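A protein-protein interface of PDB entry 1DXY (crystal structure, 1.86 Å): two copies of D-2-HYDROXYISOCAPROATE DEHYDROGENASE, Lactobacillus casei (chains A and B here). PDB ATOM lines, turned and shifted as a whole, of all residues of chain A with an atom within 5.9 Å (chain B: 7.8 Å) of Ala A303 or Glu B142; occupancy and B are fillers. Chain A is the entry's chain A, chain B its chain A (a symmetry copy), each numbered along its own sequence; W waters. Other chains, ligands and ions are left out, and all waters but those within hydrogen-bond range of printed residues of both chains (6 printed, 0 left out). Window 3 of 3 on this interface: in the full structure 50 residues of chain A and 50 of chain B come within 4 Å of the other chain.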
ATOM      1  N   TYR A 100       2.963 -31.426 -28.863  1.00  0.00           N
ATOM      2  CA  TYR A 100       2.975 -30.296 -29.785  1.00  0.00           C
ATOM      3  C   TYR A 100       2.709 -28.989 -29.031  1.00  0.00           C
ATOM      4  O   TYR A 100       3.359 -27.979 -29.298  1.00  0.00           O
ATOM      5  CB  TYR A 100       2.018 -30.490 -30.956  1.00  0.00           C
ATOM      6  CG  TYR A 100       0.731 -31.164 -30.603  1.00  0.00           C
ATOM      7  CD1 TYR A 100      -0.359 -30.430 -30.130  1.00  0.00           C
ATOM      8  CD2 TYR A 100       0.578 -32.534 -30.787  1.00  0.00           C
ATOM      9  CE1 TYR A 100      -1.574 -31.051 -29.856  1.00  0.00           C
ATOM     10  CE2 TYR A 100      -0.627 -33.169 -30.522  1.00  0.00           C
ATOM     11  CZ  TYR A 100      -1.699 -32.427 -30.060  1.00  0.00           C
ATOM     12  OH  TYR A 100      -2.901 -33.042 -29.814  1.00  0.00           O
ATOM     13  N   SER A 101       1.781 -29.018 -28.079  1.00  0.00           N
ATOM     14  CA  SER A 101       1.516 -27.839 -27.242  1.00  0.00           C
ATOM     15  C   SER A 101       0.700 -28.147 -25.996  1.00  0.00           C
ATOM     16  O   SER A 101      -0.542 -28.156 -26.025  1.00  0.00           O
ATOM     17  CB  SER A 101       0.864 -26.685 -28.026  1.00  0.00           C
ATOM     18  OG  SER A 101       0.818 -25.494 -27.247  1.00  0.00           O
ATOM     19  N   ALA A 103       0.491 -26.353 -23.535  1.00  0.00           N
ATOM     20  CA  ALA A 103      -0.086 -25.057 -23.151  1.00  0.00           C
ATOM     21  C   ALA A 103      -1.437 -24.825 -23.799  1.00  0.00           C
ATOM     22  O   ALA A 103      -2.349 -24.306 -23.158  1.00  0.00           O
ATOM     23  CB  ALA A 103       0.873 -23.916 -23.486  1.00  0.00           C
ATOM     24  N   ALA A 104      -1.597 -25.251 -25.054  1.00  0.00           N
ATOM     25  CA  ALA A 104      -2.874 -25.073 -25.744  1.00  0.00           C
ATOM     26  C   ALA A 104      -3.977 -25.757 -24.962  1.00  0.00           C
ATOM     27  O   ALA A 104      -5.037 -25.174 -24.735  1.00  0.00           O
ATOM     28  CB  ALA A 104      -2.813 -25.635 -27.173  1.00  0.00           C
ATOM     29  N   GLU A 107      -4.370 -24.173 -21.340  1.00  0.00           N
ATOM     30  CA  GLU A 107      -5.071 -22.895 -21.445  1.00  0.00           C
ATOM     31  C   GLU A 107      -6.553 -23.090 -21.707  1.00  0.00           C
ATOM     32  O   GLU A 107      -7.386 -22.358 -21.153  1.00  0.00           O
ATOM     33  CB  GLU A 107      -4.445 -21.990 -22.491  1.00  0.00           C
ATOM     34  CG  GLU A 107      -3.120 -21.411 -22.038  1.00  0.00           C
ATOM     35  CD  GLU A 107      -2.685 -20.238 -22.899  1.00  0.00           C
ATOM     36  OE1 GLU A 107      -3.515 -19.740 -23.679  1.00  0.00           O
ATOM     37  OE2 GLU A 107      -1.521 -19.803 -22.809  1.00  0.00           O
ATOM     38  N   TYR A 298      -6.678 -28.581 -28.238  1.00  0.00           N
ATOM     39  CA  TYR A 298      -5.349 -28.487 -28.830  1.00  0.00           C
ATOM     40  C   TYR A 298      -5.266 -27.385 -29.874  1.00  0.00           C
ATOM     41  O   TYR A 298      -4.191 -27.020 -30.333  1.00  0.00           O
ATOM     42  CB  TYR A 298      -5.055 -29.794 -29.600  1.00  0.00           C
ATOM     43  CG  TYR A 298      -5.718 -29.828 -30.988  1.00  0.00           C
ATOM     44  CD1 TYR A 298      -7.070 -30.137 -31.138  1.00  0.00           C
ATOM     45  CD2 TYR A 298      -5.002 -29.454 -32.134  1.00  0.00           C
ATOM     46  CE1 TYR A 298      -7.689 -30.058 -32.389  1.00  0.00           C
ATOM     47  CE2 TYR A 298      -5.604 -29.374 -33.373  1.00  0.00           C
ATOM     48  CZ  TYR A 298      -6.945 -29.670 -33.493  1.00  0.00           C
ATOM     49  OH  TYR A 298      -7.543 -29.517 -34.715  1.00  0.00           O
ATOM     50  N   TYR A 299      -6.434 -26.945 -30.300  1.00  0.00           N
ATOM     51  CA  TYR A 299      -6.584 -26.049 -31.419  1.00  0.00           C
ATOM     52  C   TYR A 299      -6.119 -24.600 -31.369  1.00  0.00           C
ATOM     53  O   TYR A 299      -6.930 -23.673 -31.363  1.00  0.00           O
ATOM     54  CB  TYR A 299      -8.037 -26.178 -31.869  1.00  0.00           C
ATOM     55  CG  TYR A 299      -8.366 -25.783 -33.274  1.00  0.00           C
ATOM     56  CD1 TYR A 299      -7.476 -26.007 -34.332  1.00  0.00           C
ATOM     57  CD2 TYR A 299      -9.592 -25.209 -33.555  1.00  0.00           C
ATOM     58  CE1 TYR A 299      -7.819 -25.661 -35.638  1.00  0.00           C
ATOM     59  CE2 TYR A 299      -9.937 -24.860 -34.841  1.00  0.00           C
ATOM     60  CZ  TYR A 299      -9.055 -25.082 -35.875  1.00  0.00           C
ATOM     61  OH  TYR A 299      -9.427 -24.657 -37.127  1.00  0.00           O
ATOM     62  N   THR A 300      -4.809 -24.403 -31.401  1.00  0.00           N
ATOM     63  CA  THR A 300      -4.264 -23.053 -31.419  1.00  0.00           C
ATOM     64  C   THR A 300      -3.261 -22.977 -32.561  1.00  0.00           C
ATOM     65  O   THR A 300      -2.787 -24.003 -33.060  1.00  0.00           O
ATOM     66  CB  THR A 300      -3.554 -22.672 -30.092  1.00  0.00           C
ATOM     67  OG1 THR A 300      -2.348 -23.426 -29.951  1.00  0.00           O
ATOM     68  CG2 THR A 300      -4.430 -22.943 -28.903  1.00  0.00           C
ATOM     69  N   GLU A 301      -2.934 -21.767 -32.982  1.00  0.00           N
ATOM     70  CA  GLU A 301      -1.978 -21.593 -34.045  1.00  0.00           C
ATOM     71  C   GLU A 301      -0.637 -22.205 -33.687  1.00  0.00           C
ATOM     72  O   GLU A 301       0.009 -22.790 -34.546  1.00  0.00           O
ATOM     73  CB  GLU A 301      -1.794 -20.126 -34.349  1.00  0.00           C
ATOM     74  CG  GLU A 301      -3.035 -19.508 -34.858  1.00  0.00           C
ATOM     75  CD  GLU A 301      -2.875 -18.025 -35.127  1.00  0.00           C
ATOM     76  OE1 GLU A 301      -1.952 -17.374 -34.551  1.00  0.00           O
ATOM     77  OE2 GLU A 301      -3.701 -17.512 -35.920  1.00  0.00           O
ATOM     78  N   THR A 302      -0.190 -22.023 -32.445  1.00  0.00           N
ATOM     79  CA  THR A 302       1.086 -22.581 -31.999  1.00  0.00           C
ATOM     80  C   THR A 302       1.075 -24.114 -32.072  1.00  0.00           C
ATOM     81  O   THR A 302       2.004 -24.714 -32.602  1.00  0.00           O
ATOM     82  CB  THR A 302       1.402 -22.128 -30.553  1.00  0.00           C
ATOM     83  OG1 THR A 302       1.347 -20.704 -30.515  1.00  0.00           O
ATOM     84  CG2 THR A 302       2.795 -22.574 -30.108  1.00  0.00           C
ATOM     85  N   ALA A 303       0.018 -24.739 -31.560  1.00  0.00           N
ATOM     86  CA  ALA A 303      -0.097 -26.200 -31.586  1.00  0.00           C
ATOM     87  C   ALA A 303      -0.082 -26.753 -33.025  1.00  0.00           C
ATOM     88  O   ALA A 303       0.686 -27.664 -33.334  1.00  0.00           O
ATOM     89  CB  ALA A 303      -1.360 -26.636 -30.874  1.00  0.00           C
ATOM     90  N   VAL A 304      -0.896 -26.178 -33.905  1.00  0.00           N
ATOM     91  CA  VAL A 304      -0.967 -26.637 -35.286  1.00  0.00           C
ATOM     92  C   VAL A 304       0.374 -26.433 -35.994  1.00  0.00           C
ATOM     93  O   VAL A 304       0.829 -27.299 -36.759  1.00  0.00           O
ATOM     94  CB  VAL A 304      -2.105 -25.940 -36.056  1.00  0.00           C
ATOM     95  CG1 VAL A 304      -2.044 -26.309 -37.537  1.00  0.00           C
ATOM     96  CG2 VAL A 304      -3.445 -26.325 -35.458  1.00  0.00           C
ATOM     97  N   HIS A 305       1.020 -25.296 -35.731  1.00  0.00           N
ATOM     98  CA  HIS A 305       2.324 -25.019 -36.308  1.00  0.00           C
ATOM     99  C   HIS A 305       3.311 -26.105 -35.855  1.00  0.00           C
ATOM    100  O   HIS A 305       4.122 -26.592 -36.648  1.00  0.00           O
ATOM    101  CB  HIS A 305       2.825 -23.641 -35.852  1.00  0.00           C
ATOM    102  CG  HIS A 305       4.267 -23.384 -36.171  1.00  0.00           C
ATOM    103  ND1 HIS A 305       4.670 -22.600 -37.231  1.00  0.00           N
ATOM    104  CD2 HIS A 305       5.402 -23.862 -35.609  1.00  0.00           C
ATOM    105  CE1 HIS A 305       5.989 -22.617 -37.318  1.00  0.00           C
ATOM    106  NE2 HIS A 305       6.455 -23.379 -36.346  1.00  0.00           N
ATOM    107  N   ASN A 306       3.265 -26.459 -34.575  1.00  0.00           N
ATOM    108  CA  ASN A 306       4.163 -27.466 -34.017  1.00  0.00           C
ATOM    109  C   ASN A 306       3.880 -28.893 -34.519  1.00  0.00           C
ATOM    110  O   ASN A 306       4.798 -29.689 -34.707  1.00  0.00           O
ATOM    111  CB  ASN A 306       4.133 -27.407 -32.491  1.00  0.00           C
ATOM    112  CG  ASN A 306       4.880 -26.197 -31.939  1.00  0.00           C
ATOM    113  OD1 ASN A 306       5.546 -25.456 -32.678  1.00  0.00           O
ATOM    114  ND2 ASN A 306       4.780 -25.998 -30.647  1.00  0.00           N
ATOM    115  N   MET A 307       2.611 -29.202 -34.730  1.00  0.00           N
ATOM    116  CA  MET A 307       2.221 -30.502 -35.244  1.00  0.00           C
ATOM    117  C   MET A 307       2.913 -30.681 -36.584  1.00  0.00           C
ATOM    118  O   MET A 307       3.516 -31.717 -36.838  1.00  0.00           O
ATOM    119  CB  MET A 307       0.718 -30.558 -35.428  1.00  0.00           C
ATOM    120  CG  MET A 307       0.001 -30.732 -34.121  1.00  0.00           C
ATOM    121  SD  MET A 307      -1.777 -30.613 -34.273  1.00  0.00           S
ATOM    122  CE  MET A 307      -2.292 -32.361 -34.260  1.00  0.00           C
ATOM    123  N   VAL A 308       2.868 -29.648 -37.416  1.00  0.00           N
ATOM    124  CA  VAL A 308       3.502 -29.694 -38.715  1.00  0.00           C
ATOM    125  C   VAL A 308       5.016 -29.715 -38.602  1.00  0.00           C
ATOM    126  O   VAL A 308       5.651 -30.689 -39.010  1.00  0.00           O
ATOM    127  CB  VAL A 308       3.079 -28.503 -39.596  1.00  0.00           C
ATOM    128  CG1 VAL A 308       3.865 -28.496 -40.913  1.00  0.00           C
ATOM    129  CG2 VAL A 308       1.589 -28.552 -39.855  1.00  0.00           C
ATOM    130  N   LEU B 114      -9.483 -15.140 -22.582  1.00  0.00           N
ATOM    131  CA  LEU B 114      -9.386 -16.535 -22.994  1.00  0.00           C
ATOM    132  C   LEU B 114     -10.581 -16.915 -23.851  1.00  0.00           C
ATOM    133  O   LEU B 114     -10.420 -17.531 -24.895  1.00  0.00           O
ATOM    134  CB  LEU B 114      -9.263 -17.436 -21.769  1.00  0.00           C
ATOM    135  CG  LEU B 114      -7.915 -17.305 -21.059  1.00  0.00           C
ATOM    136  CD1 LEU B 114      -7.953 -18.074 -19.766  1.00  0.00           C
ATOM    137  CD2 LEU B 114      -6.812 -17.831 -21.954  1.00  0.00           C
ATOM    138  N   LEU B 117      -9.829 -15.461 -27.205  1.00  0.00           N
ATOM    139  CA  LEU B 117      -8.666 -16.070 -27.850  1.00  0.00           C
ATOM    140  C   LEU B 117      -9.005 -17.467 -28.402  1.00  0.00           C
ATOM    141  O   LEU B 117      -8.409 -17.914 -29.383  1.00  0.00           O
ATOM    142  CB  LEU B 117      -7.498 -16.159 -26.868  1.00  0.00           C
ATOM    143  CG  LEU B 117      -6.721 -14.871 -26.603  1.00  0.00           C
ATOM    144  CD1 LEU B 117      -5.643 -15.164 -25.579  1.00  0.00           C
ATOM    145  CD2 LEU B 117      -6.107 -14.323 -27.882  1.00  0.00           C
ATOM    146  N   ARG B 118      -9.953 -18.144 -27.759  1.00  0.00           N
ATOM    147  CA  ARG B 118     -10.365 -19.476 -28.181  1.00  0.00           C
ATOM    148  C   ARG B 118     -11.663 -19.437 -29.000  1.00  0.00           C
ATOM    149  O   ARG B 118     -12.239 -20.485 -29.321  1.00  0.00           O
ATOM    150  CB  ARG B 118     -10.512 -20.399 -26.966  1.00  0.00           C
ATOM    151  CG  ARG B 118      -9.229 -20.537 -26.141  1.00  0.00           C
ATOM    152  CD  ARG B 118      -8.019 -20.905 -27.012  1.00  0.00           C
ATOM    153  NE  ARG B 118      -8.101 -22.284 -27.511  1.00  0.00           N
ATOM    154  CZ  ARG B 118      -7.411 -23.309 -27.013  1.00  0.00           C
ATOM    155  NH1 ARG B 118      -6.530 -23.134 -26.045  1.00  0.00           N
ATOM    156  NH2 ARG B 118      -7.573 -24.516 -27.526  1.00  0.00           N
ATOM    157  N   ILE B 139      -9.625 -21.555 -35.390  1.00  0.00           N
ATOM    158  CA  ILE B 139      -8.361 -21.744 -34.697  1.00  0.00           C
ATOM    159  C   ILE B 139      -8.098 -20.657 -33.655  1.00  0.00           C
ATOM    160  O   ILE B 139      -8.321 -19.478 -33.914  1.00  0.00           O
ATOM    161  CB  ILE B 139      -7.185 -21.896 -35.693  1.00  0.00           C
ATOM    162  CG1 ILE B 139      -5.971 -22.499 -34.978  1.00  0.00           C
ATOM    163  CG2 ILE B 139      -6.865 -20.582 -36.362  1.00  0.00           C
ATOM    164  CD1 ILE B 139      -4.895 -22.977 -35.929  1.00  0.00           C
ATOM    165  N   GLY B 140      -7.699 -21.074 -32.462  1.00  0.00           N
ATOM    166  CA  GLY B 140      -7.451 -20.125 -31.395  1.00  0.00           C
ATOM    167  C   GLY B 140      -6.004 -19.720 -31.246  1.00  0.00           C
ATOM    168  O   GLY B 140      -5.141 -20.062 -32.077  1.00  0.00           O
ATOM    169  N   LYS B 141      -5.728 -18.976 -30.182  1.00  0.00           N
ATOM    170  CA  LYS B 141      -4.374 -18.522 -29.906  1.00  0.00           C
ATOM    171  C   LYS B 141      -4.063 -18.730 -28.447  1.00  0.00           C
ATOM    172  O   LYS B 141      -4.960 -18.756 -27.595  1.00  0.00           O
ATOM    173  CB  LYS B 141      -4.212 -17.047 -30.263  1.00  0.00           C
ATOM    174  CG  LYS B 141      -4.074 -16.808 -31.727  1.00  0.00           C
ATOM    175  CD  LYS B 141      -4.783 -15.558 -32.112  1.00  0.00           C
ATOM    176  CE  LYS B 141      -3.909 -14.359 -31.964  1.00  0.00           C
ATOM    177  NZ  LYS B 141      -3.741 -13.740 -33.317  1.00  0.00           N
ATOM    178  N   GLU B 142      -2.787 -18.906 -28.162  1.00  0.00           N
ATOM    179  CA  GLU B 142      -2.342 -19.112 -26.805  1.00  0.00           C
ATOM    180  C   GLU B 142      -1.982 -17.777 -26.183  1.00  0.00           C
ATOM    181  O   GLU B 142      -1.216 -17.006 -26.762  1.00  0.00           O
ATOM    182  CB  GLU B 142      -1.120 -20.032 -26.793  1.00  0.00           C
ATOM    183  CG  GLU B 142      -1.521 -21.478 -27.021  1.00  0.00           C
ATOM    184  CD  GLU B 142      -0.354 -22.399 -27.238  1.00  0.00           C
ATOM    185  OE1 GLU B 142       0.710 -22.198 -26.621  1.00  0.00           O
ATOM    186  OE2 GLU B 142      -0.517 -23.331 -28.045  1.00  0.00           O
ATOM    187  N   LEU B 143      -2.546 -17.512 -25.015  1.00  0.00           N
ATOM    188  CA  LEU B 143      -2.273 -16.280 -24.276  1.00  0.00           C
ATOM    189  C   LEU B 143      -0.774 -16.160 -23.997  1.00  0.00           C
ATOM    190  O   LEU B 143      -0.195 -15.077 -24.098  1.00  0.00           O
ATOM    191  CB  LEU B 143      -3.070 -16.277 -22.970  1.00  0.00           C
ATOM    192  CG  LEU B 143      -2.911 -15.027 -22.110  1.00  0.00           C
ATOM    193  CD1 LEU B 143      -3.126 -13.769 -22.964  1.00  0.00           C
ATOM    194  CD2 LEU B 143      -3.941 -15.118 -21.001  1.00  0.00           C
ATOM    195  N   GLY B 144      -0.135 -17.298 -23.727  1.00  0.00           N
ATOM    196  CA  GLY B 144       1.290 -17.307 -23.458  1.00  0.00           C
ATOM    197  C   GLY B 144       2.138 -16.882 -24.643  1.00  0.00           C
ATOM    198  O   GLY B 144       3.317 -16.603 -24.488  1.00  0.00           O
ATOM    199  N   GLN B 145       1.558 -16.826 -25.831  1.00  0.00           N
ATOM    200  CA  GLN B 145       2.309 -16.413 -27.008  1.00  0.00           C
ATOM    201  C   GLN B 145       1.982 -14.964 -27.426  1.00  0.00           C
ATOM    202  O   GLN B 145       2.512 -14.460 -28.410  1.00  0.00           O
ATOM    203  CB  GLN B 145       2.012 -17.366 -28.174  1.00  0.00           C
ATOM    204  CG  GLN B 145       2.377 -18.819 -27.882  1.00  0.00           C
ATOM    205  CD  GLN B 145       3.855 -18.995 -27.615  1.00  0.00           C
ATOM    206  OE1 GLN B 145       4.688 -18.544 -28.396  1.00  0.00           O
ATOM    207  NE2 GLN B 145       4.189 -19.639 -26.508  1.00  0.00           N
ATOM    208  N   GLN B 146       1.139 -14.288 -26.659  1.00  0.00           N
ATOM    209  CA  GLN B 146       0.739 -12.929 -26.995  1.00  0.00           C
ATOM    210  C   GLN B 146       1.499 -11.853 -26.243  1.00  0.00           C
ATOM    211  O   GLN B 146       2.175 -12.121 -25.247  1.00  0.00           O
ATOM    212  CB  GLN B 146      -0.734 -12.735 -26.644  1.00  0.00           C
ATOM    213  CG  GLN B 146      -1.662 -13.782 -27.188  1.00  0.00           C
ATOM    214  CD  GLN B 146      -1.396 -14.062 -28.646  1.00  0.00           C
ATOM    215  OE1 GLN B 146      -1.058 -15.186 -29.027  1.00  0.00           O
ATOM    216  NE2 GLN B 146      -1.554 -13.053 -29.473  1.00  0.00           N
ATOM    217  N   THR B 147       1.366 -10.624 -26.740  1.00  0.00           N
ATOM    218  CA  THR B 147       1.919  -9.446 -26.085  1.00  0.00           C
ATOM    219  C   THR B 147       0.642  -8.776 -25.588  1.00  0.00           C
ATOM    220  O   THR B 147      -0.276  -8.527 -26.378  1.00  0.00           O
ATOM    221  CB  THR B 147       2.614  -8.498 -27.045  1.00  0.00           C
ATOM    222  OG1 THR B 147       3.823  -9.101 -27.508  1.00  0.00           O
ATOM    223  CG2 THR B 147       2.983  -7.208 -26.316  1.00  0.00           C
ATOM    224  N   VAL B 148       0.536  -8.609 -24.276  1.00  0.00           N
ATOM    225  CA  VAL B 148      -0.636  -7.999 -23.663  1.00  0.00           C
ATOM    226  C   VAL B 148      -0.276  -6.577 -23.180  1.00  0.00           C
ATOM    227  O   VAL B 148       0.746  -6.382 -22.501  1.00  0.00           O
ATOM    228  CB  VAL B 148      -1.115  -8.841 -22.439  1.00  0.00           C
ATOM    229  CG1 VAL B 148      -2.325  -8.197 -21.764  1.00  0.00           C
ATOM    230  CG2 VAL B 148      -1.452 -10.271 -22.874  1.00  0.00           C
ATOM    231  N   PHE B 167       0.751 -16.663 -17.474  1.00  0.00           N
ATOM    232  CA  PHE B 167       0.567 -17.471 -18.673  1.00  0.00           C
ATOM    233  C   PHE B 167       1.807 -17.460 -19.542  1.00  0.00           C
ATOM    234  O   PHE B 167       1.876 -18.177 -20.533  1.00  0.00           O
ATOM    235  CB  PHE B 167      -0.613 -16.954 -19.499  1.00  0.00           C
ATOM    236  CG  PHE B 167      -1.938 -17.360 -18.957  1.00  0.00           C
ATOM    237  CD1 PHE B 167      -2.468 -16.729 -17.836  1.00  0.00           C
ATOM    238  CD2 PHE B 167      -2.650 -18.403 -19.543  1.00  0.00           C
ATOM    239  CE1 PHE B 167      -3.673 -17.128 -17.306  1.00  0.00           C
ATOM    240  CE2 PHE B 167      -3.870 -18.818 -19.017  1.00  0.00           C
ATOM    241  CZ  PHE B 167      -4.386 -18.181 -17.892  1.00  0.00           C
ATOM    242  N   ALA B 169       2.788 -14.646 -21.042  1.00  0.00           N
ATOM    243  CA  ALA B 169       2.630 -13.578 -22.019  1.00  0.00           C
ATOM    244  C   ALA B 169       3.638 -12.476 -21.773  1.00  0.00           C
ATOM    245  O   ALA B 169       4.168 -12.339 -20.662  1.00  0.00           O
ATOM    246  CB  ALA B 169       1.232 -12.995 -21.941  1.00  0.00           C
ATOM    247  N   ASP B 199      -1.418  -7.473 -28.660  1.00  0.00           N
ATOM    248  CA  ASP B 199      -2.340  -8.412 -29.278  1.00  0.00           C
ATOM    249  C   ASP B 199      -3.642  -8.310 -28.489  1.00  0.00           C
ATOM    250  O   ASP B 199      -4.729  -8.514 -29.023  1.00  0.00           O
ATOM    251  CB  ASP B 199      -1.785  -9.823 -29.171  1.00  0.00           C
ATOM    252  CG  ASP B 199      -0.555 -10.011 -30.016  1.00  0.00           C
ATOM    253  OD1 ASP B 199      -0.673  -9.855 -31.240  1.00  0.00           O
ATOM    254  OD2 ASP B 199       0.531 -10.275 -29.474  1.00  0.00           O
ATOM    255  N   VAL B 200      -3.514  -8.017 -27.202  1.00  0.00           N
ATOM    256  CA  VAL B 200      -4.648  -7.883 -26.318  1.00  0.00           C
ATOM    257  C   VAL B 200      -4.442  -6.574 -25.564  1.00  0.00           C
ATOM    258  O   VAL B 200      -3.339  -6.317 -25.090  1.00  0.00           O
ATOM    259  CB  VAL B 200      -4.686  -9.042 -25.296  1.00  0.00           C
ATOM    260  CG1 VAL B 200      -5.836  -8.864 -24.329  1.00  0.00           C
ATOM    261  CG2 VAL B 200      -4.846 -10.368 -26.016  1.00  0.00           C
HETATM  262  O   HOH W   1      -5.266 -20.448 -25.465  1.00  0.00           O
HETATM  263  O   HOH W   2      -1.002 -19.247 -30.397  1.00  0.00           O
HETATM  264  O   HOH W   3       0.628 -20.437 -21.478  1.00  0.00           O
HETATM  265  O   HOH W   4      -9.266 -23.177 -29.920  1.00  0.00           O
HETATM  266  O   HOH W   5      -0.646 -16.904 -31.740  1.00  0.00           O
HETATM  267  O   HOH W   6       3.202 -23.212 -26.365  1.00  0.00           O
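Water W1 lies within hydrogen-bond range of the side-chain carboxylate (OE1) of Glu A107 (2.6 Å), the backbone carbonyl oxygen (O) of Lys B141 (2.7 Å) and the guanidinium group (NH1) of Arg B118 (3.0 Å). Water W3 lies within hydrogen-bond range of OE2 of Glu A107 (2.6 Å) and O of Phe B167 (2.7 Å). Water W6 bridges the side-chain carboxylate of Glu B142 (2.7 Å) and the side-chain hydroxyl of Ser A101 (3.4 Å). Water W2 lies within hydrogen-bond range of OG1 of Thr A302 and N of Glu B142. Water W4 lies within hydrogen-bond range of the backbone carbonyl oxygen (O) of Tyr A299 and the guanidinium group (NE) of Arg B118. Water W5 lies within hydrogen-bond range of the side-chain carboxylate of Glu A301 (3.1 Å) and the side-chain amide oxygen of Gln B146 (3.2 Å).
No position is printed for both chains.
Of the printed residues of chain B, Ser A101 touches Glu B142 (2.7 Å). Of the printed residues of chain B, Ala A104 touches Arg B118 and Glu B142. Of the printed residues of chain B, Glu A107 touches Glu B142, Leu B143, Gly B144 and Phe B167. Of the printed residues of chain B, Thr A300 touches Arg B118, Ile B139, Gly B140 and Glu B142. Of the printed residues of chain B, Glu A301 touches Ile B139 (3.7 Å), Gly B140 (2.9 Å) and Lys B141 (3.6 Å). Printed residues of chain B within 4 Å of Ala A303: Glu B142. Glu B142 touches seven residues of chain A. Ala B169 touches none of the printed residues of chain A. Val B200 touches none of the printed residues of chain A. The nearest residue of chain B that does not touch Ala A303 is Ile B139 (6.8 Å). The nearest residue of chain A that does not touch Glu B142 is Glu A301 (5.6 Å).
Of the 17 printed residues of chain B, 9 touch a printed residue of chain A. Of the 16 printed residues of chain A, 10 touch a printed residue of chain B. Hydrophobic or aromatic side chains of chain A that line the printed part of chain B: Ala A103, Ala A104, Tyr A299 and Val A304. Among the printed residues, 22 pairs touch across the chains. Among the printed residues, no Asp or Glu carboxylate lies within 4 Å of a Lys or Arg side-chain nitrogen of the other chain.
The backbone NH (N) of Ala A104 sits at hydrogen-bond distance from the side-chain hydroxyl (OG) of Ser A101 (3.3 Å). OG1 of Thr A300 sits at hydrogen-bond distance from N of Ala A303, at 3.1 Å. O of Leu B117 lies within hydrogen-bond range of N of Lys B141 (3.0 Å). The backbone carbonyl oxygen of Glu B142 sits close to the side-chain amide oxygen of Gln B146 (2.9 Å).
Ala A103 touches Glu B142 (CB to OE1, 3.6 Å). Ala A104 touches Glu B142 (CB to OE2, 3.4 Å). Tyr A299 touches Ile B139. Thr A300 touches Arg B118. Thr A300 touches Ile B139 (C to CG1, 3.7 Å). Glu A301 touches Lys B141 (OE1 to CG, 3.6 Å). Thr A302 touches Glu B142. Gln B145 touches Thr A302. Ala A303 touches Glu B142 (N to OE2, 3.8 Å). CG2 of Val A304 touches CD1 of Ile B139, 3.7 Å away.
OG of Ser A101 is in hydrogen-bond range of OE2 of Glu B142 (2.7 Å). The guanidinium group of Arg B118 is in hydrogen-bond range of the backbone carbonyl oxygen of Ala A104 (2.8 Å). N of Leu B143 lies within hydrogen-bond range of OE1 of Glu A107 (2.8 Å). OE2 of Glu A107 sits at hydrogen-bond distance from N of Gly B144 (3.0 Å). The backbone carbonyl oxygen (O) of Tyr A299 is in hydrogen-bond range of the backbone NH (N) of Gly B140. The side-chain hydroxyl (OG1) of Thr A300 is in hydrogen-bond range of the side-chain carboxylate (OE2) of Glu B142 (2.6 Å). The backbone NH (N) of Glu A301 sits at hydrogen-bond distance from the backbone carbonyl oxygen (O) of Gly B140 (2.9 Å).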
